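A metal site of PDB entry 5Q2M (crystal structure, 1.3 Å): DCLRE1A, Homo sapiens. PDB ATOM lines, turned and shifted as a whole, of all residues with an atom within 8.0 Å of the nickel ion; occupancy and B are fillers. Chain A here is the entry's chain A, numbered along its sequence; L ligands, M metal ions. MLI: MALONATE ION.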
ATOM      1  N   ASP A  18       4.686 -16.043 -14.877  1.00  0.00           N
ATOM      2  CA  ASP A  18       3.581 -16.681 -14.137  1.00  0.00           C
ATOM      3  C   ASP A  18       4.067 -17.798 -13.185  1.00  0.00           C
ATOM      4  O   ASP A  18       3.487 -18.848 -13.126  1.00  0.00           O
ATOM      5  CB  ASP A  18       2.477 -17.158 -15.120  1.00  0.00           C
ATOM      6  CG  ASP A  18       1.861 -15.950 -15.907  1.00  0.00           C
ATOM      7  OD1 ASP A  18       2.165 -14.760 -15.606  1.00  0.00           O
ATOM      8  OD2 ASP A  18       1.078 -16.207 -16.874  1.00  0.00           O
ATOM      9  N   THR A  34       1.536 -12.174 -16.523  1.00  0.00           N
ATOM     10  CA  THR A  34       0.800 -11.850 -17.768  1.00  0.00           C
ATOM     11  C   THR A  34      -0.560 -11.217 -17.500  1.00  0.00           C
ATOM     12  O   THR A  34      -1.018 -10.351 -18.267  1.00  0.00           O
ATOM     13  CB  THR A  34       0.675 -13.052 -18.709  1.00  0.00           C
ATOM     14  OG1 THR A  34      -0.125 -14.054 -18.057  1.00  0.00           O
ATOM     15  CG2 THR A  34       1.993 -13.611 -19.143  1.00  0.00           C
ATOM     16  N   HIS A  35      -1.260 -11.667 -16.447  1.00  0.00           N
ATOM     17  CA  HIS A  35      -2.600 -11.168 -16.176  1.00  0.00           C
ATOM     18  C   HIS A  35      -3.097 -11.605 -14.791  1.00  0.00           C
ATOM     19  O   HIS A  35      -2.550 -12.564 -14.187  1.00  0.00           O
ATOM     20  CB  HIS A  35      -3.630 -11.618 -17.269  1.00  0.00           C
ATOM     21  CG  HIS A  35      -3.954 -13.086 -17.308  1.00  0.00           C
ATOM     22  ND1 HIS A  35      -3.079 -14.066 -17.745  1.00  0.00           N
ATOM     23  CD2 HIS A  35      -5.127 -13.730 -17.108  1.00  0.00           C
ATOM     24  CE1 HIS A  35      -3.719 -15.236 -17.794  1.00  0.00           C
ATOM     25  NE2 HIS A  35      -4.946 -15.053 -17.458  1.00  0.00           N
ATOM     26  N   PHE A  36      -4.136 -10.896 -14.307  1.00  0.00           N
ATOM     27  CA  PHE A  36      -4.661 -11.115 -12.921  1.00  0.00           C
ATOM     28  C   PHE A  36      -5.761 -12.218 -12.907  1.00  0.00           C
ATOM     29  O   PHE A  36      -6.959 -11.919 -12.596  1.00  0.00           O
ATOM     30  CB  PHE A  36      -5.145  -9.807 -12.345  1.00  0.00           C
ATOM     31  CG  PHE A  36      -5.432  -9.835 -10.836  1.00  0.00           C
ATOM     32  CD1 PHE A  36      -4.367  -9.765  -9.944  1.00  0.00           C
ATOM     33  CD2 PHE A  36      -6.689  -9.807 -10.355  1.00  0.00           C
ATOM     34  CE1 PHE A  36      -4.572  -9.794  -8.558  1.00  0.00           C
ATOM     35  CE2 PHE A  36      -6.936  -9.810  -8.939  1.00  0.00           C
ATOM     36  CZ  PHE A  36      -5.866  -9.790  -8.070  1.00  0.00           C
ATOM     37  N   HIS A  37      -5.398 -13.472 -13.198  1.00  0.00           N
ATOM     38  CA  HIS A  37      -6.297 -14.677 -13.001  1.00  0.00           C
ATOM     39  C   HIS A  37      -5.490 -15.561 -11.989  1.00  0.00           C
ATOM     40  O   HIS A  37      -4.257 -15.676 -12.005  1.00  0.00           O
ATOM     41  CB  HIS A  37      -6.553 -15.416 -14.301  1.00  0.00           C
ATOM     42  CG  HIS A  37      -7.684 -14.865 -15.085  1.00  0.00           C
ATOM     43  ND1 HIS A  37      -7.884 -15.191 -16.420  1.00  0.00           N
ATOM     44  CD2 HIS A  37      -8.697 -14.023 -14.755  1.00  0.00           C
ATOM     45  CE1 HIS A  37      -8.996 -14.620 -16.834  1.00  0.00           C
ATOM     46  NE2 HIS A  37      -9.492 -13.852 -15.866  1.00  0.00           N
ATOM     47  N   SER A  38      -6.266 -16.127 -11.068  1.00  0.00           N
ATOM     48  CA  SER A  38      -5.623 -16.741  -9.873  1.00  0.00           C
ATOM     49  C   SER A  38      -4.642 -17.896 -10.139  1.00  0.00           C
ATOM     50  O   SER A  38      -3.654 -18.016  -9.397  1.00  0.00           O
ATOM     51  CB  SER A  38      -6.663 -17.152  -8.825  1.00  0.00           C
ATOM     52  OG  SER A  38      -7.550 -18.051  -9.398  1.00  0.00           O
ATOM     53  N   ASP A  39      -4.857 -18.740 -11.160  1.00  0.00           N
ATOM     54  CA  ASP A  39      -3.883 -19.808 -11.508  1.00  0.00           C
ATOM     55  C   ASP A  39      -2.527 -19.227 -11.920  1.00  0.00           C
ATOM     56  O   ASP A  39      -1.492 -19.869 -11.765  1.00  0.00           O
ATOM     57  CB  ASP A  39      -4.378 -20.752 -12.583  1.00  0.00           C
ATOM     58  CG  ASP A  39      -5.323 -21.785 -12.083  1.00  0.00           C
ATOM     59  OD1 ASP A  39      -5.578 -21.902 -10.846  1.00  0.00           O
ATOM     60  OD2 ASP A  39      -5.840 -22.519 -12.993  1.00  0.00           O
ATOM     61  N   HIS A  40      -2.524 -17.997 -12.457  1.00  0.00           N
ATOM     62  CA  HIS A  40      -1.299 -17.350 -12.921  1.00  0.00           C
ATOM     63  C   HIS A  40      -0.592 -16.583 -11.816  1.00  0.00           C
ATOM     64  O   HIS A  40       0.665 -16.562 -11.793  1.00  0.00           O
ATOM     65  CB  HIS A  40      -1.674 -16.434 -14.153  1.00  0.00           C
ATOM     66  CG  HIS A  40      -2.134 -17.245 -15.309  1.00  0.00           C
ATOM     67  ND1 HIS A  40      -1.331 -17.614 -16.361  1.00  0.00           N
ATOM     68  CD2 HIS A  40      -3.331 -17.837 -15.546  1.00  0.00           C
ATOM     69  CE1 HIS A  40      -2.003 -18.430 -17.155  1.00  0.00           C
ATOM     70  NE2 HIS A  40      -3.224 -18.538 -16.705  1.00  0.00           N
ATOM     71  N   HIS A  96      -7.516 -10.898 -23.964  1.00  0.00           N
ATOM     72  CA  HIS A  96      -8.006 -11.878 -22.950  1.00  0.00           C
ATOM     73  C   HIS A  96      -8.878 -11.044 -21.998  1.00  0.00           C
ATOM     74  O   HIS A  96      -9.876 -10.490 -22.454  1.00  0.00           O
ATOM     75  CB  HIS A  96      -6.810 -12.615 -22.367  1.00  0.00           C
ATOM     76  CG  HIS A  96      -7.129 -13.701 -21.362  1.00  0.00           C
ATOM     77  ND1 HIS A  96      -8.022 -14.715 -21.605  1.00  0.00           N
ATOM     78  CD2 HIS A  96      -6.741 -13.867 -20.053  1.00  0.00           C
ATOM     79  CE1 HIS A  96      -8.064 -15.543 -20.553  1.00  0.00           C
ATOM     80  NE2 HIS A  96      -7.293 -15.063 -19.568  1.00  0.00           N
ATOM     81  N   CYS A  97      -8.538 -10.880 -20.729  1.00  0.00           N
ATOM     82  CA  CYS A  97      -9.240 -10.029 -19.758  1.00  0.00           C
ATOM     83  C   CYS A  97      -8.546  -8.681 -19.656  1.00  0.00           C
ATOM     84  O   CYS A  97      -7.411  -8.497 -20.136  1.00  0.00           O
ATOM     85  CB  CYS A  97      -9.287 -10.797 -18.438  1.00  0.00           C
ATOM     86  SG  CYS A  97      -7.623 -11.052 -17.646  1.00  0.00           S
ATOM     87  N   ALA A 100      -4.452  -7.993 -19.491  1.00  0.00           N
ATOM     88  CA  ALA A 100      -3.703  -9.184 -19.951  1.00  0.00           C
ATOM     89  C   ALA A 100      -2.805  -8.883 -21.119  1.00  0.00           C
ATOM     90  O   ALA A 100      -3.214  -8.147 -22.071  1.00  0.00           O
ATOM     91  CB  ALA A 100      -4.642 -10.257 -20.340  1.00  0.00           C
ATOM     92  N   GLY A 117       0.992 -15.581 -22.853  1.00  0.00           N
ATOM     93  CA  GLY A 117       0.110 -15.567 -21.645  1.00  0.00           C
ATOM     94  C   GLY A 117      -1.148 -16.395 -22.011  1.00  0.00           C
ATOM     95  O   GLY A 117      -1.052 -17.361 -22.792  1.00  0.00           O
ATOM     96  N   ASP A 118      -2.308 -15.983 -21.510  1.00  0.00           N
ATOM     97  CA  ASP A 118      -3.623 -16.415 -22.022  1.00  0.00           C
ATOM     98  C   ASP A 118      -4.018 -15.375 -23.107  1.00  0.00           C
ATOM     99  O   ASP A 118      -3.879 -14.156 -22.922  1.00  0.00           O
ATOM    100  CB  ASP A 118      -4.732 -16.464 -20.994  1.00  0.00           C
ATOM    101  CG  ASP A 118      -4.686 -17.668 -20.084  1.00  0.00           C
ATOM    102  OD1 ASP A 118      -3.940 -18.637 -20.382  1.00  0.00           O
ATOM    103  OD2 ASP A 118      -5.458 -17.654 -19.045  1.00  0.00           O
ATOM    104  N   PHE A 119      -4.504 -15.880 -24.272  1.00  0.00           N
ATOM    105  CA  PHE A 119      -4.871 -14.958 -25.366  1.00  0.00           C
ATOM    106  C   PHE A 119      -6.056 -15.456 -26.205  1.00  0.00           C
ATOM    107  O   PHE A 119      -6.280 -16.667 -26.259  1.00  0.00           O
ATOM    108  CB  PHE A 119      -3.657 -14.553 -26.260  1.00  0.00           C
ATOM    109  CG  PHE A 119      -3.258 -15.478 -27.373  1.00  0.00           C
ATOM    110  CD1 PHE A 119      -2.861 -14.936 -28.610  1.00  0.00           C
ATOM    111  CD2 PHE A 119      -3.234 -16.846 -27.262  1.00  0.00           C
ATOM    112  CE1 PHE A 119      -2.470 -15.763 -29.676  1.00  0.00           C
ATOM    113  CE2 PHE A 119      -2.799 -17.685 -28.330  1.00  0.00           C
ATOM    114  CZ  PHE A 119      -2.420 -17.104 -29.510  1.00  0.00           C
ATOM    115  N   ASP A 141      -0.695 -20.374 -25.395  1.00  0.00           N
ATOM    116  CA  ASP A 141      -1.944 -20.768 -24.749  1.00  0.00           C
ATOM    117  C   ASP A 141      -2.709 -21.763 -25.624  1.00  0.00           C
ATOM    118  O   ASP A 141      -3.325 -21.372 -26.604  1.00  0.00           O
ATOM    119  CB  ASP A 141      -2.781 -19.508 -24.428  1.00  0.00           C
ATOM    120  CG  ASP A 141      -4.232 -19.784 -24.050  1.00  0.00           C
ATOM    121  OD1 ASP A 141      -4.527 -20.948 -23.668  1.00  0.00           O
ATOM    122  OD2 ASP A 141      -5.034 -18.815 -24.054  1.00  0.00           O
ATOM    123  N   THR A 143      -5.260 -23.771 -24.598  1.00  0.00           N
ATOM    124  CA  THR A 143      -6.557 -24.227 -23.955  1.00  0.00           C
ATOM    125  C   THR A 143      -7.479 -25.003 -24.935  1.00  0.00           C
ATOM    126  O   THR A 143      -8.000 -26.073 -24.567  1.00  0.00           O
ATOM    127  CB  THR A 143      -7.291 -22.970 -23.368  1.00  0.00           C
ATOM    128  OG1 THR A 143      -6.445 -22.350 -22.401  1.00  0.00           O
ATOM    129  CG2 THR A 143      -8.552 -23.390 -22.676  1.00  0.00           C
ATOM    130  N   SER A 183     -14.264 -13.783 -11.589  1.00  0.00           N
ATOM    131  CA  SER A 183     -12.905 -13.340 -11.886  1.00  0.00           C
ATOM    132  C   SER A 183     -13.120 -12.140 -12.772  1.00  0.00           C
ATOM    133  O   SER A 183     -14.246 -11.912 -13.256  1.00  0.00           O
ATOM    134  CB  SER A 183     -12.120 -14.363 -12.740  1.00  0.00           C
ATOM    135  OG  SER A 183     -12.767 -14.685 -14.005  1.00  0.00           O
ATOM    136  N   ILE A 184     -12.071 -11.413 -13.093  1.00  0.00           N
ATOM    137  CA  ILE A 184     -12.135 -10.407 -14.123  1.00  0.00           C
ATOM    138  C   ILE A 184     -12.222 -11.099 -15.504  1.00  0.00           C
ATOM    139  O   ILE A 184     -11.914 -12.267 -15.641  1.00  0.00           O
ATOM    140  CB  ILE A 184     -10.910  -9.400 -14.061  1.00  0.00           C
ATOM    141  CG1 ILE A 184      -9.549 -10.054 -14.308  1.00  0.00           C
ATOM    142  CG2 ILE A 184     -10.928  -8.659 -12.736  1.00  0.00           C
ATOM    143  CD1 ILE A 184      -8.438  -9.018 -14.482  1.00  0.00           C
ATOM    144  N   GLU A 296     -12.803 -15.833 -23.992  1.00  0.00           N
ATOM    145  CA  GLU A 296     -11.572 -15.019 -24.017  1.00  0.00           C
ATOM    146  C   GLU A 296     -10.313 -15.849 -24.282  1.00  0.00           C
ATOM    147  O   GLU A 296      -9.186 -15.383 -24.011  1.00  0.00           O
ATOM    148  CB  GLU A 296     -11.452 -14.092 -22.784  1.00  0.00           C
ATOM    149  CG  GLU A 296     -12.544 -13.024 -22.733  1.00  0.00           C
ATOM    150  CD  GLU A 296     -12.513 -12.021 -21.573  1.00  0.00           C
ATOM    151  OE1 GLU A 296     -11.883 -12.272 -20.548  1.00  0.00           O
ATOM    152  OE2 GLU A 296     -13.121 -10.918 -21.741  1.00  0.00           O
ATOM    153  N   HIS A 297     -10.478 -17.030 -24.876  1.00  0.00           N
ATOM    154  CA  HIS A 297      -9.397 -17.837 -25.424  1.00  0.00           C
ATOM    155  C   HIS A 297      -9.588 -18.072 -26.939  1.00  0.00           C
ATOM    156  O   HIS A 297     -10.746 -18.229 -27.391  1.00  0.00           O
ATOM    157  CB  HIS A 297      -9.238 -19.207 -24.727  1.00  0.00           C
ATOM    158  CG  HIS A 297      -8.836 -19.169 -23.277  1.00  0.00           C
ATOM    159  ND1 HIS A 297      -7.526 -19.028 -22.839  1.00  0.00           N
ATOM    160  CD2 HIS A 297      -9.608 -19.244 -22.172  1.00  0.00           C
ATOM    161  CE1 HIS A 297      -7.539 -19.048 -21.503  1.00  0.00           C
ATOM    162  NE2 HIS A 297      -8.784 -19.205 -21.088  1.00  0.00           N
HETATM  163  C1  MLI L   1      -7.609 -19.475 -17.227  1.00  0.00           C
HETATM  164  C2  MLI L   1      -8.637 -18.611 -17.935  1.00  0.00           C
HETATM  165  C3  MLI L   1      -6.777 -18.794 -16.194  1.00  0.00           C
HETATM  166  O6  MLI L   1      -8.337 -17.525 -18.371  1.00  0.00           O
HETATM  167  O7  MLI L   1      -9.643 -19.199 -18.330  1.00  0.00           O
HETATM  168  O8  MLI L   1      -6.570 -19.484 -15.147  1.00  0.00           O
HETATM  169  O9  MLI L   1      -6.331 -17.699 -16.457  1.00  0.00           O
HETATM  170 NI    NI M   1      -6.676 -16.323 -17.875  1.00  0.00          NI
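Within 4 Å of the nickel ion: His 35, His 37, His 96 and Asp 118.
The nearest printed residue that does not touch the nickel ion is His 40 (4.3 Å).
An oxygen (O9) of the ligand is bound to the nickel ion, at 2.0 Å.
O6 of the ligand is bound to the nickel ion, 2.1 Å away.
The nickel ion is bound by the side-chain carboxylate (OD2) of Asp 118 (2.2 Å).
A ring nitrogen (NE2) of His 35 is bound to the nickel ion, at 2.2 Å.
The nickel ion is bound by NE2 of His 96, at 2.2 Å.
The nickel ion is bound by a ring nitrogen (ND1) of His 37.
A ring nitrogen (NE2) of His 37 lies within hydrogen-bond range of the backbone carbonyl oxygen of Ile 184 (2.9 Å).
A ring nitrogen (ND1) of His 96 lies within hydrogen-bond range of the backbone carbonyl oxygen (O) of Glu 296, 2.8 Å away.
The side-chain carboxylate (OD2) of Asp 118 lies close to a ring nitrogen (NE2) of His 40 (3.4 Å).
ND1 of His 35 sits at hydrogen-bond distance from OG1 of Thr 34 (3.0 Å).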
